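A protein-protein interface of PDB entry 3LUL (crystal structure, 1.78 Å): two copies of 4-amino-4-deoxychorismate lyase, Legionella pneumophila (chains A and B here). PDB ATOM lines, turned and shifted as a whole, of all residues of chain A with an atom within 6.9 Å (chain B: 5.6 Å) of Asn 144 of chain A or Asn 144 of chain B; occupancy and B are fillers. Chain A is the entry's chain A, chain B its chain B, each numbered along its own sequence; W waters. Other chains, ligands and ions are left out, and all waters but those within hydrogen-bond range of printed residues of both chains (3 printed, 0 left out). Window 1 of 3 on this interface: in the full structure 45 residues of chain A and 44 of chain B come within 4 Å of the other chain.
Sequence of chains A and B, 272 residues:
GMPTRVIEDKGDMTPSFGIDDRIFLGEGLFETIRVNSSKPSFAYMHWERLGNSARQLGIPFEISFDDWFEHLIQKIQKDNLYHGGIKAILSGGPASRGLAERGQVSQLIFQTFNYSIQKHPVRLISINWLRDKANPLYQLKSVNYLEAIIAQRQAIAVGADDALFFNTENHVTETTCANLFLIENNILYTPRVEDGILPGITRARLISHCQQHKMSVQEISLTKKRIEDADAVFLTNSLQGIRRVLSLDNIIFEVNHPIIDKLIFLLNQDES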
ATOM      1  N   ILE A  23       4.513  -0.186 -21.517  1.00  0.00           N
ATOM      2  CA  ILE A  23       3.807  -1.236 -20.772  1.00  0.00           C
ATOM      3  C   ILE A  23       4.581  -1.645 -19.493  1.00  0.00           C
ATOM      4  O   ILE A  23       3.963  -2.057 -18.502  1.00  0.00           O
ATOM      5  CB  ILE A  23       3.485  -2.455 -21.670  1.00  0.00           C
ATOM      6  CG1 ILE A  23       2.398  -3.352 -21.021  1.00  0.00           C
ATOM      7  CG2 ILE A  23       4.800  -3.231 -22.011  1.00  0.00           C
ATOM      8  CD1 ILE A  23       1.682  -4.254 -22.042  1.00  0.00           C
ATOM      9  N   PHE A  24       5.908  -1.533 -19.503  1.00  0.00           N
ATOM     10  CA  PHE A  24       6.706  -1.879 -18.322  1.00  0.00           C
ATOM     11  C   PHE A  24       6.675  -0.845 -17.187  1.00  0.00           C
ATOM     12  O   PHE A  24       7.208  -1.107 -16.114  1.00  0.00           O
ATOM     13  CB  PHE A  24       8.125  -2.288 -18.746  1.00  0.00           C
ATOM     14  CG  PHE A  24       8.124  -3.509 -19.616  1.00  0.00           C
ATOM     15  CD1 PHE A  24       7.632  -4.716 -19.144  1.00  0.00           C
ATOM     16  CD2 PHE A  24       8.567  -3.448 -20.927  1.00  0.00           C
ATOM     17  CE1 PHE A  24       7.584  -5.857 -19.967  1.00  0.00           C
ATOM     18  CE2 PHE A  24       8.533  -4.569 -21.748  1.00  0.00           C
ATOM     19  CZ  PHE A  24       8.059  -5.779 -21.273  1.00  0.00           C
ATOM     20  N   LEU A  25       6.016   0.291 -17.450  1.00  0.00           N
ATOM     21  CA  LEU A  25       5.589   1.289 -16.469  1.00  0.00           C
ATOM     22  C   LEU A  25       4.109   1.154 -16.075  1.00  0.00           C
ATOM     23  O   LEU A  25       3.607   1.913 -15.247  1.00  0.00           O
ATOM     24  CB  LEU A  25       5.806   2.702 -17.057  1.00  0.00           C
ATOM     25  CG  LEU A  25       7.178   3.142 -17.550  1.00  0.00           C
ATOM     26  CD1 LEU A  25       7.084   4.491 -18.225  1.00  0.00           C
ATOM     27  CD2 LEU A  25       8.157   3.173 -16.389  1.00  0.00           C
ATOM     28  N   GLY A  26       3.414   0.173 -16.647  1.00  0.00           N
ATOM     29  CA  GLY A  26       1.996  -0.016 -16.395  1.00  0.00           C
ATOM     30  C   GLY A  26       1.078   0.587 -17.434  1.00  0.00           C
ATOM     31  O   GLY A  26      -0.130   0.492 -17.290  1.00  0.00           O
ATOM     32  N   GLU A  27       1.636   1.183 -18.491  1.00  0.00           N
ATOM     33  CA  GLU A  27       0.809   1.763 -19.550  1.00  0.00           C
ATOM     34  C   GLU A  27       0.407   0.719 -20.592  1.00  0.00           C
ATOM     35  O   GLU A  27       1.014   0.605 -21.688  1.00  0.00           O
ATOM     36  CB  GLU A  27       1.490   2.992 -20.159  1.00  0.00           C
ATOM     37  CG  GLU A  27       0.497   3.882 -20.939  1.00  0.00           C
ATOM     38  CD  GLU A  27       1.185   5.124 -21.469  1.00  0.00           C
ATOM     39  OE1 GLU A  27       1.935   4.987 -22.434  1.00  0.00           O
ATOM     40  OE2 GLU A  27       1.030   6.217 -20.873  1.00  0.00           O
ATOM     41  N   GLY A  28      -0.587  -0.072 -20.191  1.00  0.00           N
ATOM     42  CA  GLY A  28      -1.119  -1.132 -20.997  1.00  0.00           C
ATOM     43  C   GLY A  28      -2.524  -1.458 -20.602  1.00  0.00           C
ATOM     44  O   GLY A  28      -2.885  -1.361 -19.417  1.00  0.00           O
ATOM     45  N   PHE A  30      -5.928  -4.296 -21.555  1.00  0.00           N
ATOM     46  CA  PHE A  30      -6.264  -5.605 -22.093  1.00  0.00           C
ATOM     47  C   PHE A  30      -7.765  -5.888 -22.196  1.00  0.00           C
ATOM     48  O   PHE A  30      -8.606  -5.243 -21.540  1.00  0.00           O
ATOM     49  CB  PHE A  30      -5.521  -6.749 -21.314  1.00  0.00           C
ATOM     50  CG  PHE A  30      -6.140  -7.110 -20.023  1.00  0.00           C
ATOM     51  CD1 PHE A  30      -5.835  -6.383 -18.848  1.00  0.00           C
ATOM     52  CD2 PHE A  30      -7.027  -8.191 -19.917  1.00  0.00           C
ATOM     53  CE1 PHE A  30      -6.395  -6.715 -17.621  1.00  0.00           C
ATOM     54  CE2 PHE A  30      -7.607  -8.518 -18.691  1.00  0.00           C
ATOM     55  CZ  PHE A  30      -7.293  -7.782 -17.530  1.00  0.00           C
ATOM     56  N   LEU A 137      -7.763   4.472 -12.066  1.00  0.00           N
ATOM     57  CA  LEU A 137      -7.232   3.145 -12.350  1.00  0.00           C
ATOM     58  C   LEU A 137      -8.309   2.072 -12.344  1.00  0.00           C
ATOM     59  O   LEU A 137      -8.314   1.171 -13.177  1.00  0.00           O
ATOM     60  CB  LEU A 137      -6.172   2.772 -11.309  1.00  0.00           C
ATOM     61  CG  LEU A 137      -5.228   1.616 -11.644  1.00  0.00           C
ATOM     62  CD1 LEU A 137      -4.366   1.961 -12.865  1.00  0.00           C
ATOM     63  CD2 LEU A 137      -4.348   1.282 -10.480  1.00  0.00           C
ATOM     64  N   TYR A 138      -9.232   2.170 -11.388  1.00  0.00           N
ATOM     65  CA  TYR A 138     -10.158   1.082 -11.125  1.00  0.00           C
ATOM     66  C   TYR A 138     -11.286   0.904 -12.130  1.00  0.00           C
ATOM     67  O   TYR A 138     -12.032  -0.095 -12.077  1.00  0.00           O
ATOM     68  CB  TYR A 138     -10.675   1.168  -9.691  1.00  0.00           C
ATOM     69  CG  TYR A 138      -9.540   1.089  -8.688  1.00  0.00           C
ATOM     70  CD1 TYR A 138      -8.753  -0.064  -8.572  1.00  0.00           C
ATOM     71  CD2 TYR A 138      -9.233   2.172  -7.873  1.00  0.00           C
ATOM     72  CE1 TYR A 138      -7.712  -0.132  -7.672  1.00  0.00           C
ATOM     73  CE2 TYR A 138      -8.194   2.110  -6.966  1.00  0.00           C
ATOM     74  CZ  TYR A 138      -7.430   0.955  -6.872  1.00  0.00           C
ATOM     75  OH  TYR A 138      -6.402   0.922  -5.959  1.00  0.00           O
ATOM     76  N1  LLP A 141     -13.556  -6.933 -12.663  1.00  0.00           N
ATOM     77  C2  LLP A 141     -12.234  -7.047 -13.007  1.00  0.00           C
ATOM     78  C2' LLP A 141     -11.250  -6.735 -11.913  1.00  0.00           C
ATOM     79  C3  LLP A 141     -11.865  -7.351 -14.326  1.00  0.00           C
ATOM     80  O3  LLP A 141     -10.642  -7.386 -14.617  1.00  0.00           O
ATOM     81  C4  LLP A 141     -12.883  -7.615 -15.308  1.00  0.00           C
ATOM     82  C4' LLP A 141     -12.580  -7.923 -16.768  1.00  0.00           C
ATOM     83  C5  LLP A 141     -14.232  -7.574 -14.889  1.00  0.00           C
ATOM     84  C6  LLP A 141     -14.528  -7.215 -13.584  1.00  0.00           C
ATOM     85  C5' LLP A 141     -15.428  -7.732 -15.803  1.00  0.00           C
ATOM     86  OP4 LLP A 141     -15.441  -8.719 -16.814  1.00  0.00           O
ATOM     87  P   LLP A 141     -16.133  -8.820 -18.246  1.00  0.00           P
ATOM     88  OP1 LLP A 141     -15.941  -7.541 -19.010  1.00  0.00           O
ATOM     89  OP2 LLP A 141     -15.328  -9.980 -18.686  1.00  0.00           O
ATOM     90  OP3 LLP A 141     -17.559  -9.157 -17.900  1.00  0.00           O
ATOM     91  N   LLP A 141      -9.328  -1.673 -17.521  1.00  0.00           N
ATOM     92  CA  LLP A 141      -8.815  -3.027 -17.552  1.00  0.00           C
ATOM     93  CB  LLP A 141      -9.694  -3.864 -18.472  1.00  0.00           C
ATOM     94  CG  LLP A 141      -9.678  -5.301 -18.214  1.00  0.00           C
ATOM     95  CD  LLP A 141     -10.885  -5.982 -18.917  1.00  0.00           C
ATOM     96  CE  LLP A 141     -11.036  -7.456 -18.564  1.00  0.00           C
ATOM     97  NZ  LLP A 141     -11.304  -7.658 -17.117  1.00  0.00           N
ATOM     98  C   LLP A 141      -7.356  -2.942 -18.009  1.00  0.00           C
ATOM     99  O   LLP A 141      -7.025  -3.092 -19.179  1.00  0.00           O
ATOM    100  N   SER A 142      -6.496  -2.621 -17.060  1.00  0.00           N
ATOM    101  CA  SER A 142      -5.064  -2.371 -17.322  1.00  0.00           C
ATOM    102  C   SER A 142      -4.197  -3.535 -16.895  1.00  0.00           C
ATOM    103  O   SER A 142      -4.656  -4.488 -16.224  1.00  0.00           O
ATOM    104  CB  SER A 142      -4.636  -1.086 -16.607  1.00  0.00           C
ATOM    105  OG  SER A 142      -4.459  -1.314 -15.220  1.00  0.00           O
ATOM    106  N   VAL A 143      -2.914  -3.429 -17.218  1.00  0.00           N
ATOM    107  CA  VAL A 143      -1.904  -4.414 -16.789  1.00  0.00           C
ATOM    108  C   VAL A 143      -1.482  -4.253 -15.334  1.00  0.00           C
ATOM    109  O   VAL A 143      -0.637  -4.981 -14.811  1.00  0.00           O
ATOM    110  CB  VAL A 143      -0.691  -4.374 -17.731  1.00  0.00           C
ATOM    111  CG1 VAL A 143      -1.128  -4.821 -19.149  1.00  0.00           C
ATOM    112  CG2 VAL A 143      -0.019  -2.978 -17.756  1.00  0.00           C
ATOM    113  N   ASN A 144      -2.074  -3.287 -14.649  1.00  0.00           N
ATOM    114  CA  ASN A 144      -1.680  -2.964 -13.270  1.00  0.00           C
ATOM    115  C   ASN A 144      -2.450  -3.799 -12.262  1.00  0.00           C
ATOM    116  O   ASN A 144      -3.209  -3.240 -11.437  1.00  0.00           O
ATOM    117  CB  ASN A 144      -1.894  -1.483 -12.959  1.00  0.00           C
ATOM    118  CG  ASN A 144      -1.057  -0.560 -13.822  1.00  0.00           C
ATOM    119  OD1 ASN A 144      -0.092   0.080 -13.339  1.00  0.00           O
ATOM    120  ND2 ASN A 144      -1.478  -0.385 -15.052  1.00  0.00           N
ATOM    121  N   TYR A 145      -2.275  -5.120 -12.310  1.00  0.00           N
ATOM    122  CA  TYR A 145      -3.049  -6.048 -11.468  1.00  0.00           C
ATOM    123  C   TYR A 145      -2.327  -6.627 -10.236  1.00  0.00           C
ATOM    124  O   TYR A 145      -2.779  -7.623  -9.693  1.00  0.00           O
ATOM    125  CB  TYR A 145      -3.677  -7.161 -12.336  1.00  0.00           C
ATOM    126  CG  TYR A 145      -5.057  -6.783 -12.835  1.00  0.00           C
ATOM    127  CD1 TYR A 145      -5.306  -5.487 -13.328  1.00  0.00           C
ATOM    128  CD2 TYR A 145      -6.121  -7.687 -12.812  1.00  0.00           C
ATOM    129  CE1 TYR A 145      -6.587  -5.086 -13.811  1.00  0.00           C
ATOM    130  CE2 TYR A 145      -7.434  -7.300 -13.308  1.00  0.00           C
ATOM    131  CZ  TYR A 145      -7.639  -5.997 -13.794  1.00  0.00           C
ATOM    132  OH  TYR A 145      -8.875  -5.553 -14.259  1.00  0.00           O
ATOM    133  N   LEU A 146      -1.250  -5.983  -9.774  1.00  0.00           N
ATOM    134  CA  LEU A 146      -0.563  -6.484  -8.592  1.00  0.00           C
ATOM    135  C   LEU A 146      -1.437  -6.456  -7.329  1.00  0.00           C
ATOM    136  O   LEU A 146      -1.405  -7.396  -6.511  1.00  0.00           O
ATOM    137  CB  LEU A 146       0.778  -5.773  -8.356  1.00  0.00           C
ATOM    138  CG  LEU A 146       1.699  -6.384  -7.292  1.00  0.00           C
ATOM    139  CD1 LEU A 146       1.954  -7.934  -7.474  1.00  0.00           C
ATOM    140  CD2 LEU A 146       3.024  -5.627  -7.252  1.00  0.00           C
ATOM    141  N   GLU A 147      -2.231  -5.406  -7.173  1.00  0.00           N
ATOM    142  CA  GLU A 147      -3.207  -5.353  -6.077  1.00  0.00           C
ATOM    143  C   GLU A 147      -4.098  -6.584  -6.077  1.00  0.00           C
ATOM    144  O   GLU A 147      -4.275  -7.222  -5.048  1.00  0.00           O
ATOM    145  CB  GLU A 147      -4.054  -4.066  -6.196  1.00  0.00           C
ATOM    146  CG  GLU A 147      -4.502  -3.515  -4.964  1.00  0.00           C
ATOM    147  CD  GLU A 147      -5.384  -2.266  -5.126  1.00  0.00           C
ATOM    148  OE1 GLU A 147      -4.955  -1.251  -5.729  1.00  0.00           O
ATOM    149  OE2 GLU A 147      -6.430  -2.299  -4.493  1.00  0.00           O
ATOM    150  N   ALA A 148      -4.637  -6.940  -7.239  1.00  0.00           N
ATOM    151  CA  ALA A 148      -5.476  -8.112  -7.372  1.00  0.00           C
ATOM    152  C   ALA A 148      -4.728  -9.406  -7.102  1.00  0.00           C
ATOM    153  O   ALA A 148      -5.268 -10.297  -6.458  1.00  0.00           O
ATOM    154  CB  ALA A 148      -6.102  -8.179  -8.787  1.00  0.00           C
ATOM    155  N   ILE A 149      -3.502  -9.529  -7.614  1.00  0.00           N
ATOM    156  CA  ILE A 149      -2.636 -10.698  -7.302  1.00  0.00           C
ATOM    157  C   ILE A 149      -2.436 -10.919  -5.775  1.00  0.00           C
ATOM    158  O   ILE A 149      -2.661 -12.014  -5.276  1.00  0.00           O
ATOM    159  CB  ILE A 149      -1.269 -10.601  -8.023  1.00  0.00           C
ATOM    160  CG1 ILE A 149      -1.449 -10.753  -9.537  1.00  0.00           C
ATOM    161  CG2 ILE A 149      -0.294 -11.662  -7.507  1.00  0.00           C
ATOM    162  CD1 ILE A 149      -0.228 -10.315 -10.325  1.00  0.00           C
ATOM    163  N   LEU B  25       0.915  -8.883 -15.883  1.00  0.00           N
ATOM    164  CA  LEU B  25      -0.165  -8.781 -14.917  1.00  0.00           C
ATOM    165  C   LEU B  25       0.198  -7.779 -13.812  1.00  0.00           C
ATOM    166  O   LEU B  25      -0.578  -7.526 -12.861  1.00  0.00           O
ATOM    167  CB  LEU B  25      -0.413 -10.174 -14.292  1.00  0.00           C
ATOM    168  CG  LEU B  25      -0.632 -11.377 -15.213  1.00  0.00           C
ATOM    169  CD1 LEU B  25      -0.847 -12.675 -14.439  1.00  0.00           C
ATOM    170  CD2 LEU B  25      -1.821 -11.082 -16.094  1.00  0.00           C
ATOM    171  N   GLY B  26       1.391  -7.198 -13.910  1.00  0.00           N
ATOM    172  CA  GLY B  26       1.887  -6.293 -12.906  1.00  0.00           C
ATOM    173  C   GLY B  26       2.838  -6.898 -11.891  1.00  0.00           C
ATOM    174  O   GLY B  26       3.217  -6.206 -10.942  1.00  0.00           O
ATOM    175  N   GLU B  27       3.206  -8.163 -12.063  1.00  0.00           N
ATOM    176  CA  GLU B  27       4.075  -8.843 -11.107  1.00  0.00           C
ATOM    177  C   GLU B  27       5.525  -8.548 -11.489  1.00  0.00           C
ATOM    178  O   GLU B  27       6.191  -9.339 -12.167  1.00  0.00           O
ATOM    179  CB  GLU B  27       3.785 -10.355 -10.965  1.00  0.00           C
ATOM    180  CG  GLU B  27       4.393 -10.924  -9.694  1.00  0.00           C
ATOM    181  CD  GLU B  27       4.032 -12.370  -9.528  1.00  0.00           C
ATOM    182  OE1 GLU B  27       4.579 -13.170 -10.287  1.00  0.00           O
ATOM    183  OE2 GLU B  27       3.163 -12.694  -8.712  1.00  0.00           O
ATOM    184  N   GLY B  28       5.974  -7.346 -11.102  1.00  0.00           N
ATOM    185  CA  GLY B  28       7.351  -6.912 -11.396  1.00  0.00           C
ATOM    186  C   GLY B  28       7.786  -5.788 -10.479  1.00  0.00           C
ATOM    187  O   GLY B  28       6.948  -4.987  -9.996  1.00  0.00           O
ATOM    188  N   LEU B 137       0.578  -1.858  -2.179  1.00  0.00           N
ATOM    189  CA  LEU B 137       1.183  -1.398  -3.411  1.00  0.00           C
ATOM    190  C   LEU B 137       2.087  -0.198  -3.208  1.00  0.00           C
ATOM    191  O   LEU B 137       3.126  -0.087  -3.875  1.00  0.00           O
ATOM    192  CB  LEU B 137       0.144  -1.085  -4.507  1.00  0.00           C
ATOM    193  CG  LEU B 137      -0.009  -2.171  -5.556  1.00  0.00           C
ATOM    194  CD1 LEU B 137       1.222  -2.179  -6.456  1.00  0.00           C
ATOM    195  CD2 LEU B 137      -0.245  -3.546  -4.859  1.00  0.00           C
ATOM    196  N   SER B 142       7.092  -1.039  -7.767  1.00  0.00           N
ATOM    197  CA  SER B 142       6.620  -2.012  -8.728  1.00  0.00           C
ATOM    198  C   SER B 142       6.456  -1.408 -10.089  1.00  0.00           C
ATOM    199  O   SER B 142       6.452  -0.200 -10.228  1.00  0.00           O
ATOM    200  CB  SER B 142       5.287  -2.620  -8.319  1.00  0.00           C
ATOM    201  OG  SER B 142       4.223  -1.763  -8.630  1.00  0.00           O
ATOM    202  N   VAL B 143       6.203  -2.264 -11.080  1.00  0.00           N
ATOM    203  CA  VAL B 143       5.885  -1.823 -12.434  1.00  0.00           C
ATOM    204  C   VAL B 143       4.459  -1.231 -12.565  1.00  0.00           C
ATOM    205  O   VAL B 143       4.073  -0.811 -13.639  1.00  0.00           O
ATOM    206  CB  VAL B 143       6.070  -2.955 -13.457  1.00  0.00           C
ATOM    207  CG1 VAL B 143       7.550  -3.396 -13.508  1.00  0.00           C
ATOM    208  CG2 VAL B 143       5.157  -4.172 -13.142  1.00  0.00           C
ATOM    209  N   ASN B 144       3.662  -1.187 -11.490  1.00  0.00           N
ATOM    210  CA  ASN B 144       2.255  -0.740 -11.591  1.00  0.00           C
ATOM    211  C   ASN B 144       2.167   0.804 -11.448  1.00  0.00           C
ATOM    212  O   ASN B 144       1.594   1.321 -10.481  1.00  0.00           O
ATOM    213  CB  ASN B 144       1.372  -1.434 -10.525  1.00  0.00           C
ATOM    214  CG  ASN B 144       1.336  -2.943 -10.672  1.00  0.00           C
ATOM    215  OD1 ASN B 144       0.296  -3.524 -10.989  1.00  0.00           O
ATOM    216  ND2 ASN B 144       2.470  -3.595 -10.404  1.00  0.00           N
ATOM    217  N   TYR B 145       2.781   1.530 -12.390  1.00  0.00           N
ATOM    218  CA  TYR B 145       2.885   2.989 -12.278  1.00  0.00           C
ATOM    219  C   TYR B 145       1.867   3.776 -13.092  1.00  0.00           C
ATOM    220  O   TYR B 145       2.008   4.992 -13.225  1.00  0.00           O
ATOM    221  CB  TYR B 145       4.343   3.465 -12.548  1.00  0.00           C
ATOM    222  CG  TYR B 145       5.142   3.581 -11.216  1.00  0.00           C
ATOM    223  CD1 TYR B 145       5.119   2.542 -10.289  1.00  0.00           C
ATOM    224  CD2 TYR B 145       5.875   4.724 -10.890  1.00  0.00           C
ATOM    225  CE1 TYR B 145       5.831   2.606  -9.046  1.00  0.00           C
ATOM    226  CE2 TYR B 145       6.596   4.813  -9.651  1.00  0.00           C
ATOM    227  CZ  TYR B 145       6.562   3.746  -8.736  1.00  0.00           C
ATOM    228  OH  TYR B 145       7.216   3.770  -7.512  1.00  0.00           O
ATOM    229  N   LEU B 146       0.829   3.134 -13.638  1.00  0.00           N
ATOM    230  CA  LEU B 146      -0.160   3.904 -14.400  1.00  0.00           C
ATOM    231  C   LEU B 146      -0.788   5.048 -13.609  1.00  0.00           C
ATOM    232  O   LEU B 146      -1.020   6.144 -14.165  1.00  0.00           O
ATOM    233  CB  LEU B 146      -1.241   3.006 -14.992  1.00  0.00           C
ATOM    234  CG  LEU B 146      -2.224   3.617 -15.985  1.00  0.00           C
ATOM    235  CD1 LEU B 146      -1.578   4.421 -17.164  1.00  0.00           C
ATOM    236  CD2 LEU B 146      -3.164   2.500 -16.518  1.00  0.00           C
ATOM    237  N   GLU B 147      -1.060   4.790 -12.322  1.00  0.00           N
ATOM    238  CA  GLU B 147      -1.623   5.809 -11.455  1.00  0.00           C
ATOM    239  C   GLU B 147      -0.743   7.070 -11.451  1.00  0.00           C
ATOM    240  O   GLU B 147      -1.250   8.211 -11.573  1.00  0.00           O
ATOM    241  CB  GLU B 147      -1.813   5.277 -10.046  1.00  0.00           C
ATOM    242  CG  GLU B 147      -2.543   6.248  -9.151  1.00  0.00           C
ATOM    243  CD  GLU B 147      -2.647   5.785  -7.709  1.00  0.00           C
ATOM    244  OE1 GLU B 147      -2.759   4.565  -7.438  1.00  0.00           O
ATOM    245  OE2 GLU B 147      -2.670   6.693  -6.865  1.00  0.00           O
HETATM  246  O   HOH W   1      -1.093   2.201 -11.039  1.00  0.00           O
HETATM  247  O   HOH W   2      -1.951  -2.978  -8.688  1.00  0.00           O
HETATM  248  O   HOH W   3       1.731  -3.112 -14.412  1.00  0.00           O
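The backbone carbonyl oxygen (O) of Leu 25 of chain A sits at hydrogen-bond distance from the backbone NH (N) of Tyr 145 of chain B (3.0 Å). The backbone carbonyl oxygen (O) of Leu 25 of chain A lies within hydrogen-bond range of the backbone NH (N) of Leu 146 of chain B, 3.4 Å away. N of Gly 26 of chain A is in hydrogen-bond range of O of Val 143 of chain B, at 3.2 Å. O of Val 143 of chain A sits at hydrogen-bond distance from N of Gly 26 of chain B (3.1 Å). OD1 of Asn 144 of chain A lies within hydrogen-bond range of N of Tyr 145 of chain B, 3.4 Å away. The side-chain amide oxygen (OD1) of Asn 144 of chain A lies within hydrogen-bond range of the backbone NH (N) of Leu 146 of chain B (3.2 Å). N of Tyr 145 of chain A lies within hydrogen-bond range of O of Leu 25 of chain B. OD1 of Asn 144 of chain B sits at hydrogen-bond distance from N of Tyr 145 of chain A, 3.3 Å away. The backbone NH of Leu 146 of chain A lies within hydrogen-bond range of the side-chain amide oxygen of Asn 144 of chain B. The backbone carbonyl oxygen of Leu 25 of chain A lies close to the backbone carbonyl oxygen of Val 143 of chain B. The backbone carbonyl oxygen (O) of Val 143 of chain A sits close to the backbone carbonyl oxygen (O) of Leu 25 of chain B (3.2 Å).
The side-chain amide nitrogen of Asn 144 of chain A is in hydrogen-bond range of the backbone carbonyl oxygen of Gly 26 of chain A (2.8 Å). N of Val 143 of chain A is in hydrogen-bond range of O of Gly 28 of chain A. O3 of LLP 141 of chain A lies close to OH of Tyr 145 of chain A, 2.6 Å away. The side-chain hydroxyl (OG) of Ser 142 of chain A sits at hydrogen-bond distance from the side-chain amide nitrogen (ND2) of Asn 144 of chain A. The backbone carbonyl oxygen (O) of Gly 28 of chain B sits at hydrogen-bond distance from the backbone NH (N) of Val 143 of chain B (3.0 Å). N of Asn 144 of chain B lies within hydrogen-bond range of OG of Ser 142 of chain B (3.0 Å).
O of Phe 24 of chain A touches CB of Val 143 of chain B, at 3.4 Å. CB of Leu 146 of chain B touches O of Gly 26 of chain A (3.6 Å). Leu 137 of chain A touches Leu 146 of chain B (CD1 to CD2, 3.9 Å). Asn 144 of chain A touches Asn 144 of chain B (OD1 to C, 3.0 Å). O of Gly 26 of chain B touches CB of Leu 146 of chain A, at 3.6 Å. Leu 137 of chain B touches Leu 146 of chain A. Leu 146 of chain A touches Ser 142 of chain B (CD2 to CB, 3.9 Å). Leu 137 of chain B touches Glu 147 of chain A (CD2 to N, 3.6 Å). CD1 of Ile 149 of chain A touches O of Leu 25 of chain B (3.8 Å). OE2 of Glu 27 of chain B touches CG2 of Ile 149 of chain A, at 3.8 Å.
Asn 144 of chain A touches just these residues of chain B: Asn 144, Tyr 145 and Leu 146. Asn 144 of chain B touches just these residues of chain A: Asn 144, Tyr 145 and Leu 146. Of the printed residues of chain B, Val 143 of chain A touches Leu 25 and Gly 26. Printed residues of chain B within 4 Å of Tyr 145 of chain A: Leu 25 (3.0 Å) and Asn 144 (3.3 Å). Printed residues of chain A within 4 Å of Leu 137 of chain B: Leu 146 (3.97 Å) and Glu 147 (3.6 Å). Ile 23 of chain A touches none of the printed residues of chain B. The nearest residue of chain B that does not touch Asn 144 of chain A is Leu 25 of chain B (4.2 Å).
Of the 11 printed residues of chain B, 9 touch a printed residue of chain A. Hydrophobic or aromatic side chains of chain B that line the printed part of chain A: Leu 25, Leu 137, Val 143, Tyr 145 and Leu 146. Hydrophobic or aromatic side chains of chain A that line the printed part of chain B: Leu 137, Tyr 145, Leu 146 and Ile 149. Among the printed residues, no Asp or Glu carboxylate lies within 4 Å of a Lys or Arg side-chain nitrogen of the other chain.
Leu 25 of chain A touches Leu 146 of chain B, and with the chains exchanged Leu 146 of chain A touches Leu 25 of chain B. Gly 26 of chain A touches Leu 146 of chain B, and with the chains exchanged Leu 146 of chain A touches Gly 26 of chain B. Asn 144 of chain A touches its own counterpart, Asn 144 of chain B. Asn 144 of chain A touches Tyr 145 of chain B, and with the chains exchanged Tyr 145 of chain A touches Asn 144 of chain B. Of the 23 pairs that touch across the chains among the printed residues, 19 have their exchanged pair printed and touching as well.
Water W2 lies within hydrogen-bond range of the backbone NH of Glu 147 of chain A (2.9 Å), the backbone carbonyl oxygen of Asn 144 of chain A (3.0 Å), the side-chain amide oxygen of Asn 144 of chain B (3.3 Å) and the backbone NH of Leu 146 of chain A (3.3 Å). Water W1 lies within hydrogen-bond range of O of Asn 144 of chain B (2.9 Å), N of Glu 147 of chain B (2.9 Å), OD1 of Asn 144 of chain A (3.3 Å) and N of Leu 146 of chain B (3.4 Å). Water W3 bridges O of Val 143 of chain A (3.0 Å) and O of Val 143 of chain B (3.4 Å).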
